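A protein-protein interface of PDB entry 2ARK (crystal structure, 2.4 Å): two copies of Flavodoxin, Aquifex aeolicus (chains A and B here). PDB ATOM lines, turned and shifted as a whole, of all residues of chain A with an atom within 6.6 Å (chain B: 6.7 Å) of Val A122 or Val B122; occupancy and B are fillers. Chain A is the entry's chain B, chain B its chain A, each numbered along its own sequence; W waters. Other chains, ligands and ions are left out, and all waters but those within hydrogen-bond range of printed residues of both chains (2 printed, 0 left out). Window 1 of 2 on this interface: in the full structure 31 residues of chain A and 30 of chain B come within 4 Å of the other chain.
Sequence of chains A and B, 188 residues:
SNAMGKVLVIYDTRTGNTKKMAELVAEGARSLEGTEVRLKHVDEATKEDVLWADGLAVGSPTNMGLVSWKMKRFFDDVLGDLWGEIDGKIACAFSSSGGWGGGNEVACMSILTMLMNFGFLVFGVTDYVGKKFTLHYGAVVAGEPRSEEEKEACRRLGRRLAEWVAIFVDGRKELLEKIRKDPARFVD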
ATOM      1  N   LYS A  89      19.653 -19.814  22.133  1.00  0.00           N
ATOM      2  CA  LYS A  89      20.348 -21.036  22.520  1.00  0.00           C
ATOM      3  C   LYS A  89      19.324 -22.167  22.486  1.00  0.00           C
ATOM      4  O   LYS A  89      18.108 -21.927  22.583  1.00  0.00           O
ATOM      5  CB  LYS A  89      21.027 -20.897  23.882  1.00  0.00           C
ATOM      6  CG  LYS A  89      22.027 -19.769  23.890  1.00  0.00           C
ATOM      7  CD  LYS A  89      23.062 -19.915  24.955  1.00  0.00           C
ATOM      8  CE  LYS A  89      24.058 -18.765  24.861  1.00  0.00           C
ATOM      9  NZ  LYS A  89      25.167 -19.054  23.881  1.00  0.00           N
ATOM     10  N   ILE A  90      19.804 -23.385  22.251  1.00  0.00           N
ATOM     11  CA  ILE A  90      18.917 -24.555  22.222  1.00  0.00           C
ATOM     12  C   ILE A  90      19.059 -25.282  23.563  1.00  0.00           C
ATOM     13  O   ILE A  90      20.168 -25.390  24.097  1.00  0.00           O
ATOM     14  CB  ILE A  90      19.211 -25.502  21.013  1.00  0.00           C
ATOM     15  CG1 ILE A  90      19.112 -24.726  19.687  1.00  0.00           C
ATOM     16  CG2 ILE A  90      18.238 -26.693  21.040  1.00  0.00           C
ATOM     17  CD1 ILE A  90      19.729 -25.414  18.500  1.00  0.00           C
ATOM     18  N   ALA A  91      17.949 -25.758  24.122  1.00  0.00           N
ATOM     19  CA  ALA A  91      18.016 -26.319  25.470  1.00  0.00           C
ATOM     20  C   ALA A  91      16.976 -27.388  25.749  1.00  0.00           C
ATOM     21  O   ALA A  91      15.912 -27.424  25.138  1.00  0.00           O
ATOM     22  CB  ALA A  91      17.937 -25.186  26.513  1.00  0.00           C
ATOM     23  N   CYS A  92      17.299 -28.268  26.693  1.00  0.00           N
ATOM     24  CA  CYS A  92      16.412 -29.357  27.078  1.00  0.00           C
ATOM     25  C   CYS A  92      16.716 -29.650  28.540  1.00  0.00           C
ATOM     26  O   CYS A  92      17.581 -28.996  29.120  1.00  0.00           O
ATOM     27  CB  CYS A  92      16.667 -30.568  26.188  1.00  0.00           C
ATOM     28  SG  CYS A  92      18.361 -31.200  26.295  1.00  0.00           S
ATOM     29  N   ILE A 111      12.056 -26.627  34.580  1.00  0.00           N
ATOM     30  CA  ILE A 111      13.320 -26.347  33.905  1.00  0.00           C
ATOM     31  C   ILE A 111      13.099 -25.684  32.540  1.00  0.00           C
ATOM     32  O   ILE A 111      13.716 -24.663  32.241  1.00  0.00           O
ATOM     33  CB  ILE A 111      14.152 -27.618  33.762  1.00  0.00           C
ATOM     34  CG1 ILE A 111      14.700 -28.023  35.142  1.00  0.00           C
ATOM     35  CG2 ILE A 111      15.309 -27.374  32.815  1.00  0.00           C
ATOM     36  CD1 ILE A 111      15.033 -29.505  35.304  1.00  0.00           C
ATOM     37  N   LEU A 112      12.173 -26.239  31.752  1.00  0.00           N
ATOM     38  CA  LEU A 112      11.849 -25.717  30.433  1.00  0.00           C
ATOM     39  C   LEU A 112      11.216 -24.324  30.454  1.00  0.00           C
ATOM     40  O   LEU A 112      11.401 -23.542  29.539  1.00  0.00           O
ATOM     41  CB  LEU A 112      10.929 -26.692  29.688  1.00  0.00           C
ATOM     42  CG  LEU A 112      11.514 -28.037  29.272  1.00  0.00           C
ATOM     43  CD1 LEU A 112      10.408 -28.874  28.660  1.00  0.00           C
ATOM     44  CD2 LEU A 112      12.700 -27.950  28.319  1.00  0.00           C
ATOM     45  N   THR A 113      10.449 -24.043  31.492  1.00  0.00           N
ATOM     46  CA  THR A 113       9.825 -22.763  31.713  1.00  0.00           C
ATOM     47  C   THR A 113      10.886 -21.722  31.924  1.00  0.00           C
ATOM     48  O   THR A 113      10.796 -20.617  31.407  1.00  0.00           O
ATOM     49  CB  THR A 113       8.955 -22.846  32.980  1.00  0.00           C
ATOM     50  OG1 THR A 113       7.880 -23.735  32.714  1.00  0.00           O
ATOM     51  CG2 THR A 113       8.394 -21.485  33.420  1.00  0.00           C
ATOM     52  N   LEU A 115      14.185 -22.000  31.078  1.00  0.00           N
ATOM     53  CA  LEU A 115      14.945 -21.825  29.850  1.00  0.00           C
ATOM     54  C   LEU A 115      14.229 -21.008  28.762  1.00  0.00           C
ATOM     55  O   LEU A 115      14.852 -20.191  28.102  1.00  0.00           O
ATOM     56  CB  LEU A 115      15.331 -23.187  29.273  1.00  0.00           C
ATOM     57  CG  LEU A 115      16.182 -24.078  30.154  1.00  0.00           C
ATOM     58  CD1 LEU A 115      16.015 -25.552  29.704  1.00  0.00           C
ATOM     59  CD2 LEU A 115      17.651 -23.609  30.156  1.00  0.00           C
ATOM     60  N   MET A 116      12.932 -21.232  28.570  1.00  0.00           N
ATOM     61  CA  MET A 116      12.123 -20.409  27.668  1.00  0.00           C
ATOM     62  C   MET A 116      12.117 -18.940  28.044  1.00  0.00           C
ATOM     63  O   MET A 116      12.030 -18.073  27.173  1.00  0.00           O
ATOM     64  CB  MET A 116      10.686 -20.925  27.574  1.00  0.00           C
ATOM     65  CG  MET A 116      10.564 -22.186  26.764  1.00  0.00           C
ATOM     66  SD  MET A 116       8.669 -22.641  26.406  1.00  0.00           S
ATOM     67  CE  MET A 116       8.289 -23.859  28.034  1.00  0.00           C
ATOM     68  N   PHE A 120      15.451 -19.133  24.899  1.00  0.00           N
ATOM     69  CA  PHE A 120      15.934 -20.372  24.339  1.00  0.00           C
ATOM     70  C   PHE A 120      14.818 -21.109  23.574  1.00  0.00           C
ATOM     71  O   PHE A 120      13.614 -20.963  23.875  1.00  0.00           O
ATOM     72  CB  PHE A 120      16.490 -21.291  25.438  1.00  0.00           C
ATOM     73  CG  PHE A 120      17.660 -20.719  26.209  1.00  0.00           C
ATOM     74  CD1 PHE A 120      18.244 -19.500  25.861  1.00  0.00           C
ATOM     75  CD2 PHE A 120      18.194 -21.427  27.269  1.00  0.00           C
ATOM     76  CE1 PHE A 120      19.330 -18.984  26.585  1.00  0.00           C
ATOM     77  CE2 PHE A 120      19.301 -20.926  27.996  1.00  0.00           C
ATOM     78  CZ  PHE A 120      19.865 -19.693  27.643  1.00  0.00           C
ATOM     79  N   LEU A 121      15.242 -21.882  22.572  1.00  0.00           N
ATOM     80  CA  LEU A 121      14.381 -22.797  21.829  1.00  0.00           C
ATOM     81  C   LEU A 121      14.567 -24.085  22.540  1.00  0.00           C
ATOM     82  O   LEU A 121      15.674 -24.495  22.784  1.00  0.00           O
ATOM     83  CB  LEU A 121      14.841 -22.979  20.396  1.00  0.00           C
ATOM     84  CG  LEU A 121      14.846 -21.827  19.379  1.00  0.00           C
ATOM     85  CD1 LEU A 121      13.739 -22.020  18.384  1.00  0.00           C
ATOM     86  CD2 LEU A 121      14.803 -20.427  19.995  1.00  0.00           C
ATOM     87  N   VAL A 122      13.475 -24.741  22.859  1.00  0.00           N
ATOM     88  CA  VAL A 122      13.466 -25.754  23.900  1.00  0.00           C
ATOM     89  C   VAL A 122      12.767 -26.967  23.302  1.00  0.00           C
ATOM     90  O   VAL A 122      11.854 -26.825  22.477  1.00  0.00           O
ATOM     91  CB  VAL A 122      12.729 -25.053  25.129  1.00  0.00           C
ATOM     92  CG1 VAL A 122      11.382 -25.690  25.584  1.00  0.00           C
ATOM     93  CG2 VAL A 122      13.726 -24.625  26.212  1.00  0.00           C
ATOM     94  N   PHE A 123      13.191 -28.161  23.681  1.00  0.00           N
ATOM     95  CA  PHE A 123      12.584 -29.352  23.095  1.00  0.00           C
ATOM     96  C   PHE A 123      12.593 -30.534  24.074  1.00  0.00           C
ATOM     97  O   PHE A 123      13.338 -30.524  25.074  1.00  0.00           O
ATOM     98  CB  PHE A 123      13.336 -29.741  21.813  1.00  0.00           C
ATOM     99  CG  PHE A 123      14.720 -30.225  22.087  1.00  0.00           C
ATOM    100  CD1 PHE A 123      15.756 -29.314  22.288  1.00  0.00           C
ATOM    101  CD2 PHE A 123      14.986 -31.593  22.197  1.00  0.00           C
ATOM    102  CE1 PHE A 123      17.031 -29.745  22.599  1.00  0.00           C
ATOM    103  CE2 PHE A 123      16.251 -32.035  22.478  1.00  0.00           C
ATOM    104  CZ  PHE A 123      17.289 -31.105  22.697  1.00  0.00           C
ATOM    105  N   GLY A 124      11.771 -31.547  23.767  1.00  0.00           N
ATOM    106  CA  GLY A 124      11.966 -32.939  24.307  1.00  0.00           C
ATOM    107  C   GLY A 124      12.157 -33.945  23.161  1.00  0.00           C
ATOM    108  O   GLY A 124      12.286 -33.556  21.998  1.00  0.00           O
ATOM    109  N   LYS B  89      10.706 -29.067  13.755  1.00  0.00           N
ATOM    110  CA  LYS B  89      10.008 -27.859  13.337  1.00  0.00           C
ATOM    111  C   LYS B  89      10.094 -26.913  14.502  1.00  0.00           C
ATOM    112  O   LYS B  89      10.280 -27.359  15.635  1.00  0.00           O
ATOM    113  CB  LYS B  89       8.552 -28.123  12.931  1.00  0.00           C
ATOM    114  CG  LYS B  89       8.444 -28.643  11.525  1.00  0.00           C
ATOM    115  CD  LYS B  89       7.038 -29.050  11.156  1.00  0.00           C
ATOM    116  CE  LYS B  89       7.103 -30.087  10.043  1.00  0.00           C
ATOM    117  NZ  LYS B  89       7.802 -29.559   8.848  1.00  0.00           N
ATOM    118  N   ILE B  90       9.999 -25.616  14.212  1.00  0.00           N
ATOM    119  CA  ILE B  90      10.077 -24.561  15.208  1.00  0.00           C
ATOM    120  C   ILE B  90       8.669 -24.020  15.400  1.00  0.00           C
ATOM    121  O   ILE B  90       7.970 -23.766  14.411  1.00  0.00           O
ATOM    122  CB  ILE B  90      11.056 -23.444  14.757  1.00  0.00           C
ATOM    123  CG1 ILE B  90      12.474 -24.023  14.635  1.00  0.00           C
ATOM    124  CG2 ILE B  90      11.038 -22.273  15.726  1.00  0.00           C
ATOM    125  CD1 ILE B  90      13.461 -23.157  13.919  1.00  0.00           C
ATOM    126  N   ALA B  91       8.238 -23.885  16.662  1.00  0.00           N
ATOM    127  CA  ALA B  91       6.862 -23.485  16.984  1.00  0.00           C
ATOM    128  C   ALA B  91       6.773 -22.600  18.219  1.00  0.00           C
ATOM    129  O   ALA B  91       7.658 -22.616  19.066  1.00  0.00           O
ATOM    130  CB  ALA B  91       5.967 -24.705  17.158  1.00  0.00           C
ATOM    131  N   CYS B  92       5.699 -21.808  18.276  1.00  0.00           N
ATOM    132  CA  CYS B  92       5.301 -20.985  19.435  1.00  0.00           C
ATOM    133  C   CYS B  92       3.763 -20.965  19.512  1.00  0.00           C
ATOM    134  O   CYS B  92       3.104 -21.614  18.693  1.00  0.00           O
ATOM    135  CB  CYS B  92       5.847 -19.577  19.281  1.00  0.00           C
ATOM    136  SG  CYS B  92       5.335 -18.773  17.721  1.00  0.00           S
ATOM    137  N   ILE B 111      -0.457 -25.422  24.787  1.00  0.00           N
ATOM    138  CA  ILE B 111      -0.119 -25.445  23.364  1.00  0.00           C
ATOM    139  C   ILE B 111       1.353 -25.909  23.202  1.00  0.00           C
ATOM    140  O   ILE B 111       1.626 -26.883  22.479  1.00  0.00           O
ATOM    141  CB  ILE B 111      -0.361 -24.058  22.671  1.00  0.00           C
ATOM    142  CG1 ILE B 111      -1.854 -23.738  22.567  1.00  0.00           C
ATOM    143  CG2 ILE B 111       0.290 -24.019  21.273  1.00  0.00           C
ATOM    144  CD1 ILE B 111      -2.194 -22.276  22.252  1.00  0.00           C
ATOM    145  N   LEU B 112       2.278 -25.236  23.901  1.00  0.00           N
ATOM    146  CA  LEU B 112       3.689 -25.591  23.877  1.00  0.00           C
ATOM    147  C   LEU B 112       3.960 -27.064  24.240  1.00  0.00           C
ATOM    148  O   LEU B 112       4.834 -27.700  23.655  1.00  0.00           O
ATOM    149  CB  LEU B 112       4.515 -24.641  24.764  1.00  0.00           C
ATOM    150  CG  LEU B 112       4.579 -23.185  24.263  1.00  0.00           C
ATOM    151  CD1 LEU B 112       5.174 -22.237  25.335  1.00  0.00           C
ATOM    152  CD2 LEU B 112       5.293 -23.025  22.928  1.00  0.00           C
ATOM    153  N   THR B 113       3.206 -27.613  25.183  1.00  0.00           N
ATOM    154  CA  THR B 113       3.426 -28.986  25.577  1.00  0.00           C
ATOM    155  C   THR B 113       2.975 -29.962  24.521  1.00  0.00           C
ATOM    156  O   THR B 113       3.573 -31.011  24.326  1.00  0.00           O
ATOM    157  CB  THR B 113       2.957 -29.307  27.049  1.00  0.00           C
ATOM    158  OG1 THR B 113       2.056 -30.430  27.082  1.00  0.00           O
ATOM    159  CG2 THR B 113       2.344 -28.136  27.675  1.00  0.00           C
ATOM    160  N   LEU B 115       2.987 -29.128  21.266  1.00  0.00           N
ATOM    161  CA  LEU B 115       3.989 -28.952  20.246  1.00  0.00           C
ATOM    162  C   LEU B 115       5.265 -29.698  20.579  1.00  0.00           C
ATOM    163  O   LEU B 115       5.873 -30.306  19.686  1.00  0.00           O
ATOM    164  CB  LEU B 115       4.290 -27.462  20.008  1.00  0.00           C
ATOM    165  CG  LEU B 115       3.111 -26.652  19.469  1.00  0.00           C
ATOM    166  CD1 LEU B 115       3.320 -25.161  19.750  1.00  0.00           C
ATOM    167  CD2 LEU B 115       2.832 -26.886  18.001  1.00  0.00           C
ATOM    168  N   MET B 116       5.678 -29.669  21.847  1.00  0.00           N
ATOM    169  CA  MET B 116       6.886 -30.377  22.242  1.00  0.00           C
ATOM    170  C   MET B 116       6.754 -31.852  22.052  1.00  0.00           C
ATOM    171  O   MET B 116       7.734 -32.549  21.757  1.00  0.00           O
ATOM    172  CB  MET B 116       7.276 -30.077  23.671  1.00  0.00           C
ATOM    173  CG  MET B 116       7.976 -28.765  23.758  1.00  0.00           C
ATOM    174  SD  MET B 116       8.685 -28.414  25.557  1.00  0.00           S
ATOM    175  CE  MET B 116       6.890 -28.133  26.560  1.00  0.00           C
ATOM    176  N   PHE B 120       9.030 -30.851  18.308  1.00  0.00           N
ATOM    177  CA  PHE B 120       9.331 -29.490  17.854  1.00  0.00           C
ATOM    178  C   PHE B 120      10.221 -28.752  18.858  1.00  0.00           C
ATOM    179  O   PHE B 120      10.233 -29.060  20.051  1.00  0.00           O
ATOM    180  CB  PHE B 120       8.043 -28.678  17.646  1.00  0.00           C
ATOM    181  CG  PHE B 120       7.102 -29.245  16.610  1.00  0.00           C
ATOM    182  CD1 PHE B 120       7.493 -30.282  15.757  1.00  0.00           C
ATOM    183  CD2 PHE B 120       5.838 -28.690  16.459  1.00  0.00           C
ATOM    184  CE1 PHE B 120       6.643 -30.769  14.785  1.00  0.00           C
ATOM    185  CE2 PHE B 120       4.952 -29.148  15.485  1.00  0.00           C
ATOM    186  CZ  PHE B 120       5.348 -30.206  14.640  1.00  0.00           C
ATOM    187  N   LEU B 121      10.979 -27.788  18.346  1.00  0.00           N
ATOM    188  CA  LEU B 121      11.729 -26.838  19.164  1.00  0.00           C
ATOM    189  C   LEU B 121      10.777 -25.661  19.393  1.00  0.00           C
ATOM    190  O   LEU B 121      10.342 -25.022  18.413  1.00  0.00           O
ATOM    191  CB  LEU B 121      12.970 -26.343  18.420  1.00  0.00           C
ATOM    192  CG  LEU B 121      14.310 -27.063  18.199  1.00  0.00           C
ATOM    193  CD1 LEU B 121      15.189 -26.908  19.417  1.00  0.00           C
ATOM    194  CD2 LEU B 121      14.204 -28.552  17.792  1.00  0.00           C
ATOM    195  N   VAL B 122      10.437 -25.388  20.661  1.00  0.00           N
ATOM    196  CA  VAL B 122       9.502 -24.313  21.012  1.00  0.00           C
ATOM    197  C   VAL B 122      10.138 -23.178  21.817  1.00  0.00           C
ATOM    198  O   VAL B 122      11.173 -23.331  22.466  1.00  0.00           O
ATOM    199  CB  VAL B 122       8.243 -24.866  21.733  1.00  0.00           C
ATOM    200  CG1 VAL B 122       7.650 -26.066  20.942  1.00  0.00           C
ATOM    201  CG2 VAL B 122       8.581 -25.288  23.170  1.00  0.00           C
ATOM    202  N   PHE B 123       9.504 -22.021  21.767  1.00  0.00           N
ATOM    203  CA  PHE B 123      10.084 -20.821  22.357  1.00  0.00           C
ATOM    204  C   PHE B 123       8.954 -19.810  22.710  1.00  0.00           C
ATOM    205  O   PHE B 123       7.823 -19.901  22.203  1.00  0.00           O
ATOM    206  CB  PHE B 123      11.086 -20.186  21.354  1.00  0.00           C
ATOM    207  CG  PHE B 123      10.417 -19.609  20.146  1.00  0.00           C
ATOM    208  CD1 PHE B 123      10.063 -20.420  19.063  1.00  0.00           C
ATOM    209  CD2 PHE B 123      10.072 -18.260  20.097  1.00  0.00           C
ATOM    210  CE1 PHE B 123       9.414 -19.869  17.935  1.00  0.00           C
ATOM    211  CE2 PHE B 123       9.416 -17.726  18.981  1.00  0.00           C
ATOM    212  CZ  PHE B 123       9.074 -18.536  17.923  1.00  0.00           C
ATOM    213  N   GLY B 124       9.305 -18.865  23.577  1.00  0.00           N
ATOM    214  CA  GLY B 124       8.550 -17.631  23.801  1.00  0.00           C
ATOM    215  C   GLY B 124       9.499 -16.465  23.537  1.00  0.00           C
ATOM    216  O   GLY B 124      10.631 -16.673  23.072  1.00  0.00           O
HETATM  217  O   HOH W   1      11.772 -18.963  24.547  1.00  0.00           O
HETATM  218  O   HOH W   2      10.144 -31.181  21.543  1.00  0.00           O
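Water W2 lies within hydrogen-bond range of O of Phe B120, N of Gly A124 and O of Met B116.
Water W1 lies within hydrogen-bond range of the backbone NH of Gly B124 (2.7 Å), the backbone carbonyl oxygen of Met A116 (2.8 Å) and the backbone carbonyl oxygen of Phe A120 (2.8 Å).
Ile A90 touches Leu B121, and with the chains exchanged Leu A121 touches Ile B90.
Leu A112 touches Met B116, and with the chains exchanged Met A116 touches Leu B112.
Phe A120 touches Val B122, and with the chains exchanged Val A122 touches Phe B120.
Val A122 touches Met B116, but with the chains exchanged Met A116 does not touch Val B122 (4.2 Å).
Of the 14 pairs that touch across the chains among the printed residues, 13 have their exchanged pair printed and touching as well.
Of the 14 printed residues of chain B, 7 touch a printed residue of chain A.
Hydrophobic or aromatic side chains of chain B within 4 Å of the printed part of chain A: Ile B90, Leu B112, Met B116, Leu B121, Val B122 and Phe B123.
Hydrophobic or aromatic side chains of chain A within 4 Å of the printed part of chain B: Ile A90, Leu A112, Met A116, Leu A121, Val A122 and Phe A123.
O of Lys B89 sits at hydrogen-bond distance from N of Leu B121, at 2.8 Å.
The backbone carbonyl oxygen (O) of Lys A89 lies within hydrogen-bond range of the backbone NH (N) of Leu A121 (2.9 Å).
The backbone NH of Phe B123 sits close to the backbone carbonyl oxygen of Ala B91 (3.3 Å).
O of Leu B115 lies close to N of Phe B120.
N of Ala A91 is in hydrogen-bond range of O of Leu A121 (2.9 Å).
The backbone carbonyl oxygen (O) of Leu A115 sits close to the backbone NH (N) of Phe A120 (3.4 Å).
Among the printed residues, pairs that only touch across the chains: Ile A90 with Leu B121 (3.5 Å), Leu A112 with Met B116 (3.6 Å), Met A116 with Leu B112 (3.7 Å), Phe A120 with Val B122 (3.7 Å), Phe A120 with Phe B123 (3.7 Å), Leu A121 with Ile B90 (3.8 Å), Leu A121 with Val B122 (3.3 Å), Leu A121 with Phe B123 (3.96 Å), Val A122 with Met B116 (3.8 Å), Val A122 with Phe B120 (3.7 Å), Val A122 with Leu B121 (3.3 Å), Phe A123 with Phe B120 (3.6 Å) and Phe A123 with Leu B121 (3.8 Å).
Printed residues of chain B within 4 Å of Leu A112: Met B116.
Of the printed residues of chain B, Phe A120 touches Val B122 (3.7 Å) and Phe B123 (3.7 Å).
Printed residues of chain B within 4 Å of Leu A121: Ile B90, Val B122 and Phe B123.
Val A122 touches four residues of chain B.
Lys B89 touches none of the printed residues of chain A.
Val B122 touches three residues of chain A.
The nearest residue of chain B that does not touch Val A122 is Phe B123 (4.9 Å).
The nearest printed residue of chain B that does not touch Leu A112 is Val B122 (6.8 Å).
N of Val B122 lies within hydrogen-bond range of O of Val A122, 2.7 Å away.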
